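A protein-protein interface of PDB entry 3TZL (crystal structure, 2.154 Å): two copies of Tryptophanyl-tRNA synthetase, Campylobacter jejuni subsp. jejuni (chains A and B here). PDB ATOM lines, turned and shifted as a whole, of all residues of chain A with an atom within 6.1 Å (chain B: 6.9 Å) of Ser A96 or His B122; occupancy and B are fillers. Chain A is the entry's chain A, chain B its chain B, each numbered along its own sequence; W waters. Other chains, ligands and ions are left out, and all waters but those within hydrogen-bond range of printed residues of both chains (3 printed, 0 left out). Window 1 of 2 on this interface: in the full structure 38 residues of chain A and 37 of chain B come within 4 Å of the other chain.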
ATOM      1  N   LEU A  91       0.482   7.309  35.131  1.00  0.00           N
ATOM      2  CA  LEU A  91      -0.431   6.974  34.046  1.00  0.00           C
ATOM      3  C   LEU A  91       0.264   7.174  32.704  1.00  0.00           C
ATOM      4  O   LEU A  91       0.129   6.363  31.777  1.00  0.00           O
ATOM      5  CB  LEU A  91      -1.714   7.806  34.144  1.00  0.00           C
ATOM      6  CG  LEU A  91      -2.685   7.641  32.979  1.00  0.00           C
ATOM      7  CD1 LEU A  91      -3.098   6.196  32.863  1.00  0.00           C
ATOM      8  CD2 LEU A  91      -3.913   8.520  33.153  1.00  0.00           C
ATOM      9  N   TYR A  92       1.031   8.254  32.620  1.00  0.00           N
ATOM     10  CA  TYR A  92       1.958   8.471  31.518  1.00  0.00           C
ATOM     11  C   TYR A  92       2.759   7.204  31.165  1.00  0.00           C
ATOM     12  O   TYR A  92       2.700   6.729  30.024  1.00  0.00           O
ATOM     13  CB  TYR A  92       2.881   9.623  31.892  1.00  0.00           C
ATOM     14  CG  TYR A  92       4.087   9.819  31.025  1.00  0.00           C
ATOM     15  CD1 TYR A  92       3.977   9.992  29.647  1.00  0.00           C
ATOM     16  CD2 TYR A  92       5.338   9.908  31.597  1.00  0.00           C
ATOM     17  CE1 TYR A  92       5.107  10.210  28.864  1.00  0.00           C
ATOM     18  CE2 TYR A  92       6.449  10.121  30.851  1.00  0.00           C
ATOM     19  CZ  TYR A  92       6.343  10.272  29.480  1.00  0.00           C
ATOM     20  OH  TYR A  92       7.492  10.488  28.767  1.00  0.00           O
ATOM     21  N   TRP A  93       3.478   6.637  32.136  1.00  0.00           N
ATOM     22  CA  TRP A  93       4.229   5.394  31.894  1.00  0.00           C
ATOM     23  C   TRP A  93       3.336   4.217  31.436  1.00  0.00           C
ATOM     24  O   TRP A  93       3.705   3.436  30.564  1.00  0.00           O
ATOM     25  CB  TRP A  93       4.988   4.955  33.148  1.00  0.00           C
ATOM     26  CG  TRP A  93       5.615   3.585  32.990  1.00  0.00           C
ATOM     27  CD1 TRP A  93       5.259   2.428  33.645  1.00  0.00           C
ATOM     28  CD2 TRP A  93       6.687   3.222  32.095  1.00  0.00           C
ATOM     29  NE1 TRP A  93       6.056   1.379  33.229  1.00  0.00           N
ATOM     30  CE2 TRP A  93       6.935   1.835  32.278  1.00  0.00           C
ATOM     31  CE3 TRP A  93       7.462   3.933  31.161  1.00  0.00           C
ATOM     32  CZ2 TRP A  93       7.918   1.146  31.554  1.00  0.00           C
ATOM     33  CZ3 TRP A  93       8.438   3.256  30.453  1.00  0.00           C
ATOM     34  CH2 TRP A  93       8.662   1.866  30.654  1.00  0.00           C
ATOM     35  N   ILE A  94       2.174   4.084  32.059  1.00  0.00           N
ATOM     36  CA  ILE A  94       1.246   3.023  31.699  1.00  0.00           C
ATOM     37  C   ILE A  94       0.709   3.217  30.280  1.00  0.00           C
ATOM     38  O   ILE A  94       0.662   2.277  29.482  1.00  0.00           O
ATOM     39  CB  ILE A  94       0.096   2.958  32.713  1.00  0.00           C
ATOM     40  CG1 ILE A  94       0.644   2.463  34.063  1.00  0.00           C
ATOM     41  CG2 ILE A  94      -1.087   2.107  32.190  1.00  0.00           C
ATOM     42  CD1 ILE A  94      -0.356   2.540  35.179  1.00  0.00           C
ATOM     43  N   LEU A  95       0.315   4.441  29.958  1.00  0.00           N
ATOM     44  CA  LEU A  95      -0.161   4.721  28.609  1.00  0.00           C
ATOM     45  C   LEU A  95       0.894   4.463  27.535  1.00  0.00           C
ATOM     46  O   LEU A  95       0.535   4.123  26.402  1.00  0.00           O
ATOM     47  CB  LEU A  95      -0.695   6.146  28.488  1.00  0.00           C
ATOM     48  CG  LEU A  95      -1.963   6.452  29.276  1.00  0.00           C
ATOM     49  CD1 LEU A  95      -2.359   7.907  29.040  1.00  0.00           C
ATOM     50  CD2 LEU A  95      -3.110   5.484  28.923  1.00  0.00           C
ATOM     51  N   SER A  96       2.182   4.588  27.873  1.00  0.00           N
ATOM     52  CA  SER A  96       3.238   4.361  26.862  1.00  0.00           C
ATOM     53  C   SER A  96       3.223   2.910  26.390  1.00  0.00           C
ATOM     54  O   SER A  96       3.756   2.586  25.323  1.00  0.00           O
ATOM     55  CB  SER A  96       4.641   4.678  27.384  1.00  0.00           C
ATOM     56  OG  SER A  96       4.819   6.048  27.678  1.00  0.00           O
ATOM     57  N   GLN A  97       2.635   2.025  27.188  1.00  0.00           N
ATOM     58  CA  GLN A  97       2.700   0.611  26.841  1.00  0.00           C
ATOM     59  C   GLN A  97       1.643   0.347  25.798  1.00  0.00           C
ATOM     60  O   GLN A  97       1.660  -0.683  25.138  1.00  0.00           O
ATOM     61  CB  GLN A  97       2.526  -0.309  28.060  1.00  0.00           C
ATOM     62  CG  GLN A  97       3.363   0.079  29.262  1.00  0.00           C
ATOM     63  CD  GLN A  97       4.805   0.400  28.924  1.00  0.00           C
ATOM     64  OE1 GLN A  97       5.421  -0.246  28.077  1.00  0.00           O
ATOM     65  NE2 GLN A  97       5.361   1.403  29.603  1.00  0.00           N
ATOM     66  N   PHE A  98       0.743   1.312  25.630  1.00  0.00           N
ATOM     67  CA  PHE A  98      -0.316   1.198  24.653  1.00  0.00           C
ATOM     68  C   PHE A  98      -0.112   2.081  23.430  1.00  0.00           C
ATOM     69  O   PHE A  98      -0.942   2.083  22.526  1.00  0.00           O
ATOM     70  CB  PHE A  98      -1.652   1.529  25.305  1.00  0.00           C
ATOM     71  CG  PHE A  98      -2.075   0.539  26.344  1.00  0.00           C
ATOM     72  CD1 PHE A  98      -2.879  -0.543  26.000  1.00  0.00           C
ATOM     73  CD2 PHE A  98      -1.675   0.687  27.667  1.00  0.00           C
ATOM     74  CE1 PHE A  98      -3.285  -1.459  26.954  1.00  0.00           C
ATOM     75  CE2 PHE A  98      -2.082  -0.224  28.634  1.00  0.00           C
ATOM     76  CZ  PHE A  98      -2.891  -1.300  28.273  1.00  0.00           C
ATOM     77  N   THR A  99       0.982   2.832  23.407  1.00  0.00           N
ATOM     78  CA  THR A  99       1.235   3.788  22.338  1.00  0.00           C
ATOM     79  C   THR A  99       2.254   3.243  21.345  1.00  0.00           C
ATOM     80  O   THR A  99       3.426   3.095  21.687  1.00  0.00           O
ATOM     81  CB  THR A  99       1.792   5.121  22.900  1.00  0.00           C
ATOM     82  OG1 THR A  99       0.983   5.558  24.004  1.00  0.00           O
ATOM     83  CG2 THR A  99       1.838   6.204  21.804  1.00  0.00           C
ATOM     84  N   PRO A 100       1.811   2.953  20.111  1.00  0.00           N
ATOM     85  CA  PRO A 100       2.721   2.571  19.026  1.00  0.00           C
ATOM     86  C   PRO A 100       3.624   3.749  18.687  1.00  0.00           C
ATOM     87  O   PRO A 100       3.134   4.871  18.631  1.00  0.00           O
ATOM     88  CB  PRO A 100       1.777   2.320  17.844  1.00  0.00           C
ATOM     89  CG  PRO A 100       0.391   2.203  18.450  1.00  0.00           C
ATOM     90  CD  PRO A 100       0.416   3.069  19.653  1.00  0.00           C
ATOM     91  N   MET A 101       4.910   3.497  18.475  1.00  0.00           N
ATOM     92  CA  MET A 101       5.844   4.559  18.088  1.00  0.00           C
ATOM     93  C   MET A 101       5.358   5.278  16.842  1.00  0.00           C
ATOM     94  O   MET A 101       5.417   6.508  16.773  1.00  0.00           O
ATOM     95  CB  MET A 101       7.249   4.002  17.865  1.00  0.00           C
ATOM     96  CG  MET A 101       7.955   3.688  19.169  1.00  0.00           C
ATOM     97  SD  MET A 101       8.435   5.380  19.994  1.00  0.00           S
ATOM     98  CE  MET A 101       9.873   5.830  18.751  1.00  0.00           C
ATOM     99  N   LEU A 104       3.536   8.375  17.204  1.00  0.00           N
ATOM    100  CA  LEU A 104       4.285   9.512  17.739  1.00  0.00           C
ATOM    101  C   LEU A 104       5.273  10.064  16.716  1.00  0.00           C
ATOM    102  O   LEU A 104       5.551  11.267  16.699  1.00  0.00           O
ATOM    103  CB  LEU A 104       5.033   9.119  19.013  1.00  0.00           C
ATOM    104  CG  LEU A 104       4.156   8.722  20.195  1.00  0.00           C
ATOM    105  CD1 LEU A 104       5.008   8.242  21.361  1.00  0.00           C
ATOM    106  CD2 LEU A 104       3.269   9.894  20.599  1.00  0.00           C
ATOM    107  N   HIS A 122      13.957  13.282  24.138  1.00  0.00           N
ATOM    108  CA  HIS A 122      12.900  12.302  24.386  1.00  0.00           C
ATOM    109  C   HIS A 122      11.665  12.974  24.954  1.00  0.00           C
ATOM    110  O   HIS A 122      10.542  12.572  24.663  1.00  0.00           O
ATOM    111  CB  HIS A 122      13.406  11.213  25.337  1.00  0.00           C
ATOM    112  CG  HIS A 122      12.396  10.152  25.640  1.00  0.00           C
ATOM    113  ND1 HIS A 122      11.812  10.014  26.883  1.00  0.00           N
ATOM    114  CD2 HIS A 122      11.861   9.184  24.860  1.00  0.00           C
ATOM    115  CE1 HIS A 122      10.971   8.991  26.860  1.00  0.00           C
ATOM    116  NE2 HIS A 122      10.983   8.472  25.644  1.00  0.00           N
ATOM    117  N   PHE A 125       9.647  14.660  22.164  1.00  0.00           N
ATOM    118  CA  PHE A 125       8.982  13.575  21.443  1.00  0.00           C
ATOM    119  C   PHE A 125       7.827  12.969  22.228  1.00  0.00           C
ATOM    120  O   PHE A 125       6.782  12.653  21.652  1.00  0.00           O
ATOM    121  CB  PHE A 125      10.000  12.489  21.122  1.00  0.00           C
ATOM    122  CG  PHE A 125       9.447  11.336  20.323  1.00  0.00           C
ATOM    123  CD1 PHE A 125       9.235  11.459  18.952  1.00  0.00           C
ATOM    124  CD2 PHE A 125       9.216  10.114  20.925  1.00  0.00           C
ATOM    125  CE1 PHE A 125       8.755  10.390  18.202  1.00  0.00           C
ATOM    126  CE2 PHE A 125       8.733   9.029  20.182  1.00  0.00           C
ATOM    127  CZ  PHE A 125       8.499   9.171  18.821  1.00  0.00           C
ATOM    128  N   SER A 126       8.012  12.820  23.542  1.00  0.00           N
ATOM    129  CA  SER A 126       7.034  12.123  24.382  1.00  0.00           C
ATOM    130  C   SER A 126       5.900  13.002  24.868  1.00  0.00           C
ATOM    131  O   SER A 126       4.938  12.499  25.448  1.00  0.00           O
ATOM    132  CB  SER A 126       7.719  11.473  25.584  1.00  0.00           C
ATOM    133  OG  SER A 126       8.732  10.615  25.113  1.00  0.00           O
ATOM    134  N   VAL A 129       2.229  11.925  24.838  1.00  0.00           N
ATOM    135  CA  VAL A 129       1.814  10.833  25.725  1.00  0.00           C
ATOM    136  C   VAL A 129       1.484  11.358  27.112  1.00  0.00           C
ATOM    137  O   VAL A 129       0.491  10.957  27.721  1.00  0.00           O
ATOM    138  CB  VAL A 129       2.866   9.722  25.834  1.00  0.00           C
ATOM    139  CG1 VAL A 129       2.320   8.565  26.683  1.00  0.00           C
ATOM    140  CG2 VAL A 129       3.250   9.225  24.471  1.00  0.00           C
ATOM    141  N   TYR B  92      12.299  10.154  35.839  1.00  0.00           N
ATOM    142  CA  TYR B  92      12.224   9.668  34.467  1.00  0.00           C
ATOM    143  C   TYR B  92      11.789  10.767  33.484  1.00  0.00           C
ATOM    144  O   TYR B  92      12.434  10.971  32.453  1.00  0.00           O
ATOM    145  CB  TYR B  92      11.289   8.456  34.446  1.00  0.00           C
ATOM    146  CG  TYR B  92      10.653   8.067  33.134  1.00  0.00           C
ATOM    147  CD1 TYR B  92      11.418   7.673  32.044  1.00  0.00           C
ATOM    148  CD2 TYR B  92       9.270   8.014  33.016  1.00  0.00           C
ATOM    149  CE1 TYR B  92      10.820   7.288  30.857  1.00  0.00           C
ATOM    150  CE2 TYR B  92       8.670   7.613  31.846  1.00  0.00           C
ATOM    151  CZ  TYR B  92       9.449   7.256  30.762  1.00  0.00           C
ATOM    152  OH  TYR B  92       8.838   6.871  29.577  1.00  0.00           O
ATOM    153  N   ALA B 120       7.033  -1.256  17.668  1.00  0.00           N
ATOM    154  CA  ALA B 120       7.453  -0.998  19.035  1.00  0.00           C
ATOM    155  C   ALA B 120       6.567   0.055  19.713  1.00  0.00           C
ATOM    156  O   ALA B 120       6.153   1.031  19.096  1.00  0.00           O
ATOM    157  CB  ALA B 120       8.921  -0.573  19.066  1.00  0.00           C
ATOM    158  N   SER B 121       6.271  -0.172  20.984  1.00  0.00           N
ATOM    159  CA  SER B 121       5.523   0.785  21.773  1.00  0.00           C
ATOM    160  C   SER B 121       6.486   1.859  22.237  1.00  0.00           C
ATOM    161  O   SER B 121       7.704   1.638  22.301  1.00  0.00           O
ATOM    162  CB  SER B 121       4.915   0.109  23.004  1.00  0.00           C
ATOM    163  OG  SER B 121       5.943  -0.274  23.916  1.00  0.00           O
ATOM    164  N   HIS B 122       5.938   3.020  22.559  1.00  0.00           N
ATOM    165  CA  HIS B 122       6.705   4.080  23.205  1.00  0.00           C
ATOM    166  C   HIS B 122       7.378   3.552  24.465  1.00  0.00           C
ATOM    167  O   HIS B 122       8.502   3.941  24.806  1.00  0.00           O
ATOM    168  CB  HIS B 122       5.767   5.211  23.597  1.00  0.00           C
ATOM    169  CG  HIS B 122       6.468   6.414  24.129  1.00  0.00           C
ATOM    170  ND1 HIS B 122       6.268   6.889  25.407  1.00  0.00           N
ATOM    171  CD2 HIS B 122       7.379   7.239  23.562  1.00  0.00           C
ATOM    172  CE1 HIS B 122       7.006   7.969  25.597  1.00  0.00           C
ATOM    173  NE2 HIS B 122       7.685   8.207  24.489  1.00  0.00           N
ATOM    174  N   GLY B 123       6.687   2.657  25.158  1.00  0.00           N
ATOM    175  CA  GLY B 123       7.215   2.063  26.374  1.00  0.00           C
ATOM    176  C   GLY B 123       8.518   1.315  26.166  1.00  0.00           C
ATOM    177  O   GLY B 123       9.448   1.480  26.944  1.00  0.00           O
ATOM    178  N   LEU B 124       8.589   0.506  25.109  1.00  0.00           N
ATOM    179  CA  LEU B 124       9.824  -0.200  24.756  1.00  0.00           C
ATOM    180  C   LEU B 124      10.942   0.769  24.410  1.00  0.00           C
ATOM    181  O   LEU B 124      12.074   0.580  24.822  1.00  0.00           O
ATOM    182  CB  LEU B 124       9.614  -1.142  23.567  1.00  0.00           C
ATOM    183  CG  LEU B 124      10.881  -1.888  23.122  1.00  0.00           C
ATOM    184  CD1 LEU B 124      11.435  -2.734  24.257  1.00  0.00           C
ATOM    185  CD2 LEU B 124      10.633  -2.744  21.896  1.00  0.00           C
ATOM    186  N   PHE B 125      10.609   1.790  23.633  1.00  0.00           N
ATOM    187  CA  PHE B 125      11.552   2.818  23.214  1.00  0.00           C
ATOM    188  C   PHE B 125      12.098   3.595  24.415  1.00  0.00           C
ATOM    189  O   PHE B 125      13.285   3.937  24.468  1.00  0.00           O
ATOM    190  CB  PHE B 125      10.824   3.779  22.266  1.00  0.00           C
ATOM    191  CG  PHE B 125      11.694   4.848  21.674  1.00  0.00           C
ATOM    192  CD1 PHE B 125      12.574   4.553  20.657  1.00  0.00           C
ATOM    193  CD2 PHE B 125      11.598   6.161  22.111  1.00  0.00           C
ATOM    194  CE1 PHE B 125      13.371   5.549  20.089  1.00  0.00           C
ATOM    195  CE2 PHE B 125      12.386   7.152  21.556  1.00  0.00           C
ATOM    196  CZ  PHE B 125      13.273   6.846  20.544  1.00  0.00           C
ATOM    197  N   SER B 126      11.226   3.858  25.382  1.00  0.00           N
ATOM    198  CA  SER B 126      11.537   4.759  26.487  1.00  0.00           C
ATOM    199  C   SER B 126      12.156   4.086  27.707  1.00  0.00           C
ATOM    200  O   SER B 126      12.703   4.761  28.572  1.00  0.00           O
ATOM    201  CB  SER B 126      10.278   5.485  26.937  1.00  0.00           C
ATOM    202  OG  SER B 126       9.658   6.143  25.850  1.00  0.00           O
ATOM    203  N   TYR B 127      12.069   2.768  27.804  1.00  0.00           N
ATOM    204  CA  TYR B 127      12.540   2.140  29.037  1.00  0.00           C
ATOM    205  C   TYR B 127      14.004   2.342  29.450  1.00  0.00           C
ATOM    206  O   TYR B 127      14.283   2.321  30.639  1.00  0.00           O
ATOM    207  CB  TYR B 127      12.093   0.684  29.156  1.00  0.00           C
ATOM    208  CG  TYR B 127      13.067  -0.354  28.680  1.00  0.00           C
ATOM    209  CD1 TYR B 127      14.096  -0.813  29.498  1.00  0.00           C
ATOM    210  CD2 TYR B 127      12.921  -0.923  27.431  1.00  0.00           C
ATOM    211  CE1 TYR B 127      14.976  -1.796  29.053  1.00  0.00           C
ATOM    212  CE2 TYR B 127      13.793  -1.897  26.978  1.00  0.00           C
ATOM    213  CZ  TYR B 127      14.812  -2.330  27.785  1.00  0.00           C
ATOM    214  OH  TYR B 127      15.644  -3.314  27.301  1.00  0.00           O
HETATM  215  O   HOH W   1       6.197   6.916  29.731  1.00  0.00           O
HETATM  216  O   HOH W   2       5.008  -1.965  25.731  1.00  0.00           O
HETATM  217  O   HOH W   3       9.781  10.499  30.392  1.00  0.00           O
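The backbone carbonyl oxygen (O) of Ala B120 is in hydrogen-bond range of the backbone NH (N) of Met A101, 2.8 Å away.
The backbone NH (N) of Gly B123 sits at hydrogen-bond distance from the backbone carbonyl oxygen (O) of Ser A96 (2.9 Å).
OG of Ser A96 is in hydrogen-bond range of ND1 of His B122 (2.8 Å).
O of Thr A99 lies within hydrogen-bond range of N of His B122, 2.7 Å away.
OG of Ser A126 sits at hydrogen-bond distance from NE2 of His B122 (2.7 Å).
OG of Ser B126 is in hydrogen-bond range of NE2 of His A122.
O of Leu A95 lies within hydrogen-bond range of OG1 of Thr A99, 2.8 Å away.
The backbone carbonyl oxygen (O) of His B122 sits at hydrogen-bond distance from the side-chain hydroxyl (OG) of Ser B126.
The backbone carbonyl oxygen (O) of His A122 is in hydrogen-bond range of the side-chain hydroxyl (OG) of Ser A126, at 2.7 Å.
The backbone carbonyl oxygen of Trp A93 lies within hydrogen-bond range of the side-chain amide nitrogen of Gln A97 (2.8 Å).
OG of Ser B121 lies within hydrogen-bond range of N of Leu B124 (3.0 Å).
The backbone carbonyl oxygen of Tyr A92 sits at hydrogen-bond distance from the side-chain hydroxyl of Ser A96 (3.2 Å).
Among the printed residues, pairs that only touch across the chains: Thr A99 with Ser B121, Gln A97 with Gly B123, Leu A104 with His B122, Tyr A92 with Tyr B92, His A122 with His B122, Met A101 with Phe B125, Ser A96 with Ser B121, Trp A93 with Tyr B92, Pro A100 with Ala B120, Met A101 with Ser B121, Trp A93 with Gly B123, Met A101 with His B122, His A122 with Phe B125, Trp A93 with Tyr B127, Val A129 with His B122 and Gln A97 with Ser B121.
Ser A96 touches three residues of chain B.
Of the printed residues of chain B, Gln A97 touches Ser B121 (3.97 Å) and Gly B123 (3.4 Å).
Of the printed residues of chain B, Pro A100 touches Ala B120.
Printed residues of chain B within 4 Å of His A122: His B122, Phe B125 and Ser B126.
Of chain A, only Ser A96 (2.8 Å), Thr A99 (2.7 Å), Met A101 (3.9 Å), Leu A104 (3.4 Å), His A122 (3.5 Å), Ser A126 (2.7 Å) and Val A129 (3.9 Å) come within 4 Å of His B122.
Of the printed residues of chain A, Phe B125 touches Met A101 (3.5 Å) and His A122 (3.9 Å).
Of the printed residues of chain A, Tyr B127 touches Trp A93 (3.9 Å).
The nearest printed residue of chain A that does not touch His B122 is Phe A125 (4.1 Å).
The nearest printed residue of chain B that does not touch Val A129 is Ser B126 (7.2 Å).
Of the 9 printed residues of chain B, 8 touch a printed residue of chain A.
Printed residues of chain B that touch a printed residue of chain A: Tyr B92, Ala B120, Ser B121, His B122, Gly B123, Phe B125, Ser B126 and Tyr B127.
Hydrophobic or aromatic side chains of chain B that line the printed part of chain A: Tyr B92, His B122, Phe B125 and Tyr B127.
Along chain B the printed residues that touch a printed residue of chain A span positions 92 to 127.
Hydrophobic or aromatic side chains of chain A within 4 Å of the printed part of chain B: Tyr A92, Trp A93, Met A101, Leu A104, His A122 and Val A129.
Among the printed residues, 22 pairs touch across the chains.
Among the printed residues, no Asp or Glu carboxylate lies within 4 Å of a Lys or Arg side-chain nitrogen of the other chain.
Tyr B92 touches its own counterpart, Tyr A92.
His A122 touches its own counterpart, His B122.
His A122 touches Phe B125, but with the chains exchanged Phe A125 does not touch His B122 (4.1 Å).
His A122 touches Ser B126, and with the chains exchanged Ser A126 touches His B122.
Positions printed for both chains: 92, 122, 125 and 126.
Of the 22 pairs that touch across the chains among the printed residues, 4 have their exchanged pair printed and touching as well.
Water W1 bridges OG of Ser A96 and OH of Tyr B92.
Water W2 lies within hydrogen-bond range of the side-chain hydroxyl of Ser B121 (2.7 Å) and the side-chain amide oxygen of Gln A97 (2.9 Å).
Water W3 bridges OH of Tyr A92 (2.8 Å) and O of Tyr B92 (3.4 Å).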
